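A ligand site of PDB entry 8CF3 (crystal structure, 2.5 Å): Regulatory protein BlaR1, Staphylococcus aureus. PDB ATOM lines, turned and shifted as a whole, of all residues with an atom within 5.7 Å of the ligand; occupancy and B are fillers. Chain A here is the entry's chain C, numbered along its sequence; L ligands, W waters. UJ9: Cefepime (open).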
ATOM      1  N   PRO A  55     -27.077   7.928 -33.530  1.00  0.00           N
ATOM      2  CA  PRO A  55     -28.185   7.299 -32.801  1.00  0.00           C
ATOM      3  C   PRO A  55     -27.937   5.859 -32.331  1.00  0.00           C
ATOM      4  O   PRO A  55     -28.698   5.344 -31.519  1.00  0.00           O
ATOM      5  CB  PRO A  55     -29.327   7.371 -33.827  1.00  0.00           C
ATOM      6  CG  PRO A  55     -28.639   7.278 -35.155  1.00  0.00           C
ATOM      7  CD  PRO A  55     -27.328   8.015 -34.975  1.00  0.00           C
ATOM      8  N   ASN A  56     -26.862   5.215 -32.828  1.00  0.00           N
ATOM      9  CA  ASN A  56     -26.560   3.835 -32.507  1.00  0.00           C
ATOM     10  C   ASN A  56     -27.799   2.971 -32.784  1.00  0.00           C
ATOM     11  O   ASN A  56     -28.406   3.068 -33.852  1.00  0.00           O
ATOM     12  CB  ASN A  56     -26.117   3.635 -31.044  1.00  0.00           C
ATOM     13  CG  ASN A  56     -24.943   4.481 -30.616  1.00  0.00           C
ATOM     14  OD1 ASN A  56     -24.969   5.080 -29.546  1.00  0.00           O
ATOM     15  ND2 ASN A  56     -23.901   4.500 -31.432  1.00  0.00           N
ATOM     16  N   SER A  57     -28.201   2.177 -31.787  1.00  0.00           N
ATOM     17  CA  SER A  57     -29.269   1.220 -31.959  1.00  0.00           C
ATOM     18  C   SER A  57     -30.674   1.778 -31.735  1.00  0.00           C
ATOM     19  O   SER A  57     -31.643   1.047 -31.894  1.00  0.00           O
ATOM     20  CB  SER A  57     -29.028   0.057 -31.018  1.00  0.00           C
ATOM     21  OG  SER A  57     -27.848  -0.602 -31.487  1.00  0.00           O
ATOM     22  N   THR A  58     -30.777   3.076 -31.398  1.00  0.00           N
ATOM     23  CA  THR A  58     -32.070   3.738 -31.332  1.00  0.00           C
ATOM     24  C   THR A  58     -32.626   3.913 -32.746  1.00  0.00           C
ATOM     25  O   THR A  58     -33.843   4.057 -32.922  1.00  0.00           O
ATOM     26  CB  THR A  58     -31.989   5.086 -30.607  1.00  0.00           C
ATOM     27  OG1 THR A  58     -31.199   5.999 -31.369  1.00  0.00           O
ATOM     28  CG2 THR A  58     -31.436   4.950 -29.211  1.00  0.00           C
ATOM     29  N   LYS A  60     -32.764   1.665 -34.848  1.00  0.00           N
ATOM     30  CA  LYS A  60     -33.520   0.441 -35.120  1.00  0.00           C
ATOM     31  C   LYS A  60     -35.021   0.693 -35.079  1.00  0.00           C
ATOM     32  O   LYS A  60     -35.776   0.042 -35.805  1.00  0.00           O
ATOM     33  CB  LYS A  60     -33.155  -0.666 -34.133  1.00  0.00           C
ATOM     34  CG  LYS A  60     -31.798  -1.310 -34.350  1.00  0.00           C
ATOM     35  CD  LYS A  60     -31.398  -2.254 -33.235  1.00  0.00           C
ATOM     36  CE  LYS A  60     -30.209  -3.114 -33.598  1.00  0.00           C
ATOM     37  NZ  LYS A  60     -29.197  -3.130 -32.529  1.00  0.00           N
ATOM     38  N   PHE A  89     -22.622 -11.681 -29.053  1.00  0.00           N
ATOM     39  CA  PHE A  89     -23.717 -11.957 -28.145  1.00  0.00           C
ATOM     40  C   PHE A  89     -24.463 -13.196 -28.625  1.00  0.00           C
ATOM     41  O   PHE A  89     -24.714 -13.343 -29.824  1.00  0.00           O
ATOM     42  CB  PHE A  89     -24.638 -10.738 -28.081  1.00  0.00           C
ATOM     43  CG  PHE A  89     -23.909  -9.432 -27.905  1.00  0.00           C
ATOM     44  CD1 PHE A  89     -23.406  -9.048 -26.674  1.00  0.00           C
ATOM     45  CD2 PHE A  89     -23.695  -8.593 -28.995  1.00  0.00           C
ATOM     46  CE1 PHE A  89     -22.726  -7.851 -26.520  1.00  0.00           C
ATOM     47  CE2 PHE A  89     -23.018  -7.386 -28.834  1.00  0.00           C
ATOM     48  CZ  PHE A  89     -22.539  -7.019 -27.597  1.00  0.00           C
ATOM     49  N   TRP A  92     -27.940 -13.171 -30.498  1.00  0.00           N
ATOM     50  CA  TRP A  92     -27.905 -12.861 -31.918  1.00  0.00           C
ATOM     51  C   TRP A  92     -27.800 -14.127 -32.771  1.00  0.00           C
ATOM     52  O   TRP A  92     -28.133 -14.095 -33.960  1.00  0.00           O
ATOM     53  CB  TRP A  92     -26.734 -11.916 -32.221  1.00  0.00           C
ATOM     54  CG  TRP A  92     -26.827 -10.574 -31.577  1.00  0.00           C
ATOM     55  CD1 TRP A  92     -27.697 -10.173 -30.601  1.00  0.00           C
ATOM     56  CD2 TRP A  92     -26.009  -9.440 -31.880  1.00  0.00           C
ATOM     57  NE1 TRP A  92     -27.469  -8.861 -30.268  1.00  0.00           N
ATOM     58  CE2 TRP A  92     -26.447  -8.381 -31.038  1.00  0.00           C
ATOM     59  CE3 TRP A  92     -24.957  -9.208 -32.764  1.00  0.00           C
ATOM     60  CZ2 TRP A  92     -25.857  -7.119 -31.075  1.00  0.00           C
ATOM     61  CZ3 TRP A  92     -24.377  -7.955 -32.803  1.00  0.00           C
ATOM     62  CH2 TRP A  92     -24.815  -6.937 -31.966  1.00  0.00           C
ATOM     63  N   SER A 105     -31.472  -6.138 -29.372  1.00  0.00           N
ATOM     64  CA  SER A 105     -30.713  -5.200 -30.191  1.00  0.00           C
ATOM     65  C   SER A 105     -29.812  -5.956 -31.170  1.00  0.00           C
ATOM     66  O   SER A 105     -28.612  -5.707 -31.269  1.00  0.00           O
ATOM     67  CB  SER A 105     -29.930  -4.251 -29.305  1.00  0.00           C
ATOM     68  OG  SER A 105     -29.673  -3.024 -29.965  1.00  0.00           O
ATOM     69  N   ASN A 107     -28.175  -6.415 -34.179  1.00  0.00           N
ATOM     70  CA  ASN A 107     -27.740  -5.542 -35.261  1.00  0.00           C
ATOM     71  C   ASN A 107     -28.062  -6.128 -36.636  1.00  0.00           C
ATOM     72  O   ASN A 107     -28.606  -5.437 -37.488  1.00  0.00           O
ATOM     73  CB  ASN A 107     -26.243  -5.224 -35.170  1.00  0.00           C
ATOM     74  CG  ASN A 107     -25.865  -4.371 -33.984  1.00  0.00           C
ATOM     75  OD1 ASN A 107     -26.713  -4.048 -33.139  1.00  0.00           O
ATOM     76  ND2 ASN A 107     -24.599  -4.004 -33.895  1.00  0.00           N
ATOM     77  N   MET A 144     -24.377   4.061 -37.291  1.00  0.00           N
ATOM     78  CA  MET A 144     -23.457   3.550 -36.281  1.00  0.00           C
ATOM     79  C   MET A 144     -22.181   4.372 -36.263  1.00  0.00           C
ATOM     80  O   MET A 144     -21.278   4.160 -37.072  1.00  0.00           O
ATOM     81  CB  MET A 144     -23.106   2.078 -36.560  1.00  0.00           C
ATOM     82  CG  MET A 144     -24.314   1.174 -36.628  1.00  0.00           C
ATOM     83  SD  MET A 144     -24.096  -0.327 -35.658  1.00  0.00           S
ATOM     84  CE  MET A 144     -25.203   0.025 -34.287  1.00  0.00           C
ATOM     85  N   GLU A 145     -22.119   5.323 -35.318  1.00  0.00           N
ATOM     86  CA  GLU A 145     -20.967   6.212 -35.150  1.00  0.00           C
ATOM     87  C   GLU A 145     -20.397   6.618 -36.514  1.00  0.00           C
ATOM     88  O   GLU A 145     -19.196   6.500 -36.743  1.00  0.00           O
ATOM     89  CB  GLU A 145     -19.931   5.548 -34.248  1.00  0.00           C
ATOM     90  CG  GLU A 145     -20.448   5.223 -32.844  1.00  0.00           C
ATOM     91  CD  GLU A 145     -20.978   6.407 -32.030  1.00  0.00           C
ATOM     92  OE1 GLU A 145     -20.323   7.477 -32.028  1.00  0.00           O
ATOM     93  OE2 GLU A 145     -22.034   6.230 -31.369  1.00  0.00           O
ATOM     94  N   LYS A 194     -35.951   1.961 -26.258  1.00  0.00           N
ATOM     95  CA  LYS A 194     -34.851   1.313 -26.948  1.00  0.00           C
ATOM     96  C   LYS A 194     -33.531   1.910 -26.478  1.00  0.00           C
ATOM     97  O   LYS A 194     -33.389   3.134 -26.451  1.00  0.00           O
ATOM     98  CB  LYS A 194     -34.989   1.494 -28.464  1.00  0.00           C
ATOM     99  CG  LYS A 194     -33.956   0.763 -29.305  1.00  0.00           C
ATOM    100  CD  LYS A 194     -34.057  -0.759 -29.179  1.00  0.00           C
ATOM    101  CE  LYS A 194     -32.869  -1.483 -29.765  1.00  0.00           C
ATOM    102  NZ  LYS A 194     -31.671  -1.356 -28.907  1.00  0.00           N
ATOM    103  N   THR A 195     -32.574   1.046 -26.152  1.00  0.00           N
ATOM    104  CA  THR A 195     -31.250   1.479 -25.710  1.00  0.00           C
ATOM    105  C   THR A 195     -30.337   1.664 -26.925  1.00  0.00           C
ATOM    106  O   THR A 195     -30.580   1.077 -27.984  1.00  0.00           O
ATOM    107  CB  THR A 195     -30.630   0.471 -24.744  1.00  0.00           C
ATOM    108  OG1 THR A 195     -30.783  -0.824 -25.320  1.00  0.00           O
ATOM    109  CG2 THR A 195     -31.262   0.515 -23.368  1.00  0.00           C
ATOM    110  N   GLY A 196     -29.311   2.494 -26.739  1.00  0.00           N
ATOM    111  CA  GLY A 196     -28.186   2.584 -27.664  1.00  0.00           C
ATOM    112  C   GLY A 196     -26.864   2.600 -26.897  1.00  0.00           C
ATOM    113  O   GLY A 196     -26.760   3.245 -25.862  1.00  0.00           O
ATOM    114  N   THR A 197     -25.886   1.851 -27.402  1.00  0.00           N
ATOM    115  CA  THR A 197     -24.560   1.848 -26.802  1.00  0.00           C
ATOM    116  C   THR A 197     -23.504   1.945 -27.891  1.00  0.00           C
ATOM    117  O   THR A 197     -23.593   1.260 -28.915  1.00  0.00           O
ATOM    118  CB  THR A 197     -24.324   0.595 -25.946  1.00  0.00           C
ATOM    119  OG1 THR A 197     -25.337   0.503 -24.950  1.00  0.00           O
ATOM    120  CG2 THR A 197     -22.971   0.587 -25.272  1.00  0.00           C
ATOM    121  N   GLY A 198     -22.518   2.805 -27.648  1.00  0.00           N
ATOM    122  CA  GLY A 198     -21.346   2.911 -28.495  1.00  0.00           C
ATOM    123  C   GLY A 198     -20.104   2.489 -27.726  1.00  0.00           C
ATOM    124  O   GLY A 198     -20.012   2.710 -26.519  1.00  0.00           O
ATOM    125  N   ILE A 199     -19.158   1.861 -28.431  1.00  0.00           N
ATOM    126  CA  ILE A 199     -17.889   1.455 -27.858  1.00  0.00           C
ATOM    127  C   ILE A 199     -16.768   1.908 -28.793  1.00  0.00           C
ATOM    128  O   ILE A 199     -16.809   1.653 -29.999  1.00  0.00           O
ATOM    129  CB  ILE A 199     -17.888  -0.070 -27.600  1.00  0.00           C
ATOM    130  CG1 ILE A 199     -16.778  -0.501 -26.642  1.00  0.00           C
ATOM    131  CG2 ILE A 199     -17.862  -0.866 -28.900  1.00  0.00           C
ATOM    132  CD1 ILE A 199     -17.100  -0.240 -25.188  1.00  0.00           C
ATOM    133  N   VAL A 200     -15.792   2.643 -28.236  1.00  0.00           N
ATOM    134  CA  VAL A 200     -14.607   3.074 -28.964  1.00  0.00           C
ATOM    135  C   VAL A 200     -13.390   2.819 -28.078  1.00  0.00           C
ATOM    136  O   VAL A 200     -13.344   3.259 -26.928  1.00  0.00           O
ATOM    137  CB  VAL A 200     -14.684   4.555 -29.402  1.00  0.00           C
ATOM    138  CG1 VAL A 200     -15.865   4.813 -30.329  1.00  0.00           C
ATOM    139  CG2 VAL A 200     -14.724   5.509 -28.226  1.00  0.00           C
ATOM    140  N   TYR A 204     -17.005   2.964 -23.406  1.00  0.00           N
ATOM    141  CA  TYR A 204     -18.309   3.510 -23.744  1.00  0.00           C
ATOM    142  C   TYR A 204     -18.173   5.005 -24.003  1.00  0.00           C
ATOM    143  O   TYR A 204     -17.546   5.703 -23.210  1.00  0.00           O
ATOM    144  CB  TYR A 204     -19.320   3.252 -22.617  1.00  0.00           C
ATOM    145  CG  TYR A 204     -19.668   1.815 -22.354  1.00  0.00           C
ATOM    146  CD1 TYR A 204     -20.014   0.957 -23.389  1.00  0.00           C
ATOM    147  CD2 TYR A 204     -19.674   1.306 -21.067  1.00  0.00           C
ATOM    148  CE1 TYR A 204     -20.339  -0.363 -23.146  1.00  0.00           C
ATOM    149  CE2 TYR A 204     -20.006  -0.011 -20.805  1.00  0.00           C
ATOM    150  CZ  TYR A 204     -20.347  -0.851 -21.852  1.00  0.00           C
ATOM    151  OH  TYR A 204     -20.675  -2.160 -21.600  1.00  0.00           O
ATOM    152  N   ASN A 205     -18.750   5.488 -25.115  1.00  0.00           N
ATOM    153  CA  ASN A 205     -18.615   6.887 -25.500  1.00  0.00           C
ATOM    154  C   ASN A 205     -19.966   7.531 -25.814  1.00  0.00           C
ATOM    155  O   ASN A 205     -20.024   8.749 -25.973  1.00  0.00           O
ATOM    156  CB  ASN A 205     -17.677   7.031 -26.700  1.00  0.00           C
ATOM    157  CG  ASN A 205     -18.197   6.344 -27.948  1.00  0.00           C
ATOM    158  OD1 ASN A 205     -18.551   5.175 -27.907  1.00  0.00           O
ATOM    159  ND2 ASN A 205     -18.257   7.071 -29.054  1.00  0.00           N
ATOM    160  N   SER A 232     -23.331   4.052 -21.239  1.00  0.00           N
ATOM    161  CA  SER A 232     -23.900   2.864 -21.857  1.00  0.00           C
ATOM    162  C   SER A 232     -25.423   2.992 -21.945  1.00  0.00           C
ATOM    163  O   SER A 232     -26.024   3.687 -21.130  1.00  0.00           O
ATOM    164  CB  SER A 232     -23.525   1.630 -21.094  1.00  0.00           C
ATOM    165  OG  SER A 232     -24.042   1.669 -19.773  1.00  0.00           O
ATOM    166  N   GLY A 233     -26.013   2.320 -22.931  1.00  0.00           N
ATOM    167  CA  GLY A 233     -27.453   2.281 -23.095  1.00  0.00           C
ATOM    168  C   GLY A 233     -28.180   1.835 -21.832  1.00  0.00           C
ATOM    169  O   GLY A 233     -29.230   2.377 -21.504  1.00  0.00           O
ATOM    170  N   LYS A 234     -27.617   0.843 -21.123  1.00  0.00           N
ATOM    171  CA  LYS A 234     -28.244   0.322 -19.912  1.00  0.00           C
ATOM    172  C   LYS A 234     -28.225   1.403 -18.829  1.00  0.00           C
ATOM    173  O   LYS A 234     -29.215   1.582 -18.109  1.00  0.00           O
ATOM    174  CB  LYS A 234     -27.550  -0.944 -19.396  1.00  0.00           C
ATOM    175  CG  LYS A 234     -28.201  -1.530 -18.152  1.00  0.00           C
ATOM    176  CD  LYS A 234     -27.623  -2.828 -17.640  1.00  0.00           C
ATOM    177  CE  LYS A 234     -28.395  -3.338 -16.437  1.00  0.00           C
ATOM    178  NZ  LYS A 234     -27.913  -4.667 -15.987  1.00  0.00           N
HETATM  179  C5  UJ9 L   1     -25.770  -1.610 -30.773  1.00  0.00           C
HETATM  180  C15 UJ9 L   1     -26.733  -0.446 -30.780  1.00  0.00           C
HETATM  181  C01 UJ9 L   1     -26.336  -2.761 -29.921  1.00  0.00           C
HETATM  182  N01 UJ9 L   1     -27.097  -2.251 -28.794  1.00  0.00           N
HETATM  183  O1  UJ9 L   1     -26.381   0.525 -29.812  1.00  0.00           O
HETATM  184  S01 UJ9 L   1     -25.068  -3.985 -29.522  1.00  0.00           S
HETATM  185  C02 UJ9 L   1     -25.200  -2.661 -25.611  1.00  0.00           C
HETATM  186  N02 UJ9 L   1     -24.435  -1.134 -30.387  1.00  0.00           N
HETATM  187  O02 UJ9 L   1     -23.394  -2.159 -32.124  1.00  0.00           O
HETATM  188  S02 UJ9 L   1     -20.980   1.798 -33.412  1.00  0.00           S
HETATM  189  C03 UJ9 L   1     -24.569  -3.374 -27.897  1.00  0.00           C
HETATM  190  N03 UJ9 L   1     -21.359  -1.110 -29.600  1.00  0.00           N
HETATM  191  O03 UJ9 L   1     -21.956  -2.106 -28.823  1.00  0.00           O
HETATM  192  C04 UJ9 L   1     -25.687  -2.963 -26.998  1.00  0.00           C
HETATM  193  N04 UJ9 L   1     -18.808   2.412 -31.953  1.00  0.00           N
HETATM  194  O04 UJ9 L   1     -27.505  -0.901 -25.719  1.00  0.00           O
HETATM  195  C05 UJ9 L   1     -26.736  -2.199 -27.555  1.00  0.00           C
HETATM  196  N05 UJ9 L   1     -25.698  -3.355 -24.330  1.00  0.00           N
HETATM  197  O05 UJ9 L   1     -29.028  -1.920 -27.013  1.00  0.00           O
HETATM  198  C06 UJ9 L   1     -26.896  -4.226 -24.634  1.00  0.00           C
HETATM  199  N06 UJ9 L   1     -20.293   0.793 -31.131  1.00  0.00           N
HETATM  200  C07 UJ9 L   1     -23.350  -1.443 -31.120  1.00  0.00           C
HETATM  201  C08 UJ9 L   1     -22.061  -0.842 -30.650  1.00  0.00           C
HETATM  202  C09 UJ9 L   1     -21.008  -2.616 -27.867  1.00  0.00           C
HETATM  203  C10 UJ9 L   1     -21.464   0.184 -31.516  1.00  0.00           C
HETATM  204  C11 UJ9 L   1     -27.810  -1.622 -26.674  1.00  0.00           C
HETATM  205  C12 UJ9 L   1     -19.909   1.670 -32.039  1.00  0.00           C
HETATM  206  C14 UJ9 L   1     -21.965   0.593 -32.698  1.00  0.00           C
HETATM  207  C22 UJ9 L   1     -24.587  -4.154 -23.682  1.00  0.00           C
HETATM  208  C23 UJ9 L   1     -23.907  -3.232 -22.657  1.00  0.00           C
HETATM  209  C24 UJ9 L   1     -24.842  -2.024 -22.436  1.00  0.00           C
HETATM  210  C25 UJ9 L   1     -26.103  -2.353 -23.255  1.00  0.00           C
HETATM  211  O   HOH W   1     -25.637  -7.109 -24.987  1.00  0.00           O
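The backbone NH (N) of Ser 57 sits close to an oxygen (O1) of the ligand, 3.2 Å away.
The side-chain hydroxyl (OG) of Ser 57 is covalently linked to a carbon (C15) of the ligand (1.3 Å).
The side-chain hydroxyl of Thr 195 lies within hydrogen-bond range of an oxygen (O05) of the ligand, 2.7 Å away.
The backbone NH (N) of Thr 197 lies within hydrogen-bond range of an oxygen (O1) of the ligand (2.8 Å).
O of Thr 197 sits at hydrogen-bond distance from N02 of the ligand, 2.9 Å away.
The side-chain hydroxyl (OG1) of Thr 197 is in hydrogen-bond range of an oxygen (O04) of the ligand (2.7 Å).
ND2 of Asn 107 is in hydrogen-bond range of O02 of the ligand, at 2.8 Å.
The backbone NH of Ile 199 is in hydrogen-bond range of a nitrogen (N06) of the ligand, at 3.1 Å.
O of Ile 199 is in hydrogen-bond range of N04 of the ligand.
OG of Ser 105 is in hydrogen-bond range of N01 of the ligand (2.9 Å).
The side-chain amino group of Lys 194 is in salt-bridge range of an oxygen (O05) of the ligand.
The side-chain hydroxyl of Ser 57 sits close to the side-chain hydroxyl of Ser 105, 3.4 Å away.
OG of Ser 57 lies within hydrogen-bond range of NZ of Lys 60 (3.0 Å).
The backbone NH (N) of Gly 233 is in hydrogen-bond range of the side-chain hydroxyl (OG1) of Thr 197, at 2.8 Å.
N of Ile 199 is in hydrogen-bond range of OD1 of Asn 205.
OG of Ser 105 sits at hydrogen-bond distance from NZ of Lys 194 (2.8 Å).
The side-chain amino group (NZ) of Lys 60 lies within hydrogen-bond range of the side-chain hydroxyl (OG) of Ser 105 (2.6 Å).
The side-chain amide nitrogen (ND2) of Asn 56 lies within hydrogen-bond range of the side-chain carboxylate (OE2) of Glu 145 (2.5 Å).
The backbone carbonyl oxygen (O) of Gly 196 sits close to the backbone NH (N) of Gly 233, at 3.2 Å.
CB of Asn 56 touches O1 of the ligand, 3.4 Å away.
Lys 60 touches the ligand.
Trp 92 touches the ligand.
CE of Met 144 touches O02 of the ligand, at 3.6 Å.
Glu 145 touches the ligand (CG to N04, 3.4 Å).
Gly 196 touches the ligand (CA to O1, 3.5 Å).
Gly 198 touches the ligand (CA to N06, 3.5 Å).
OH of Tyr 204 touches C23 of the ligand (3.6 Å).
Within 4 Å of the ligand: Asn 56, Ser 57, Lys 60, Trp 92, Ser 105, Asn 107, Met 144, Glu 145, Lys 194, Thr 195, Gly 196, Thr 197, Gly 198, Ile 199 and Tyr 204.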
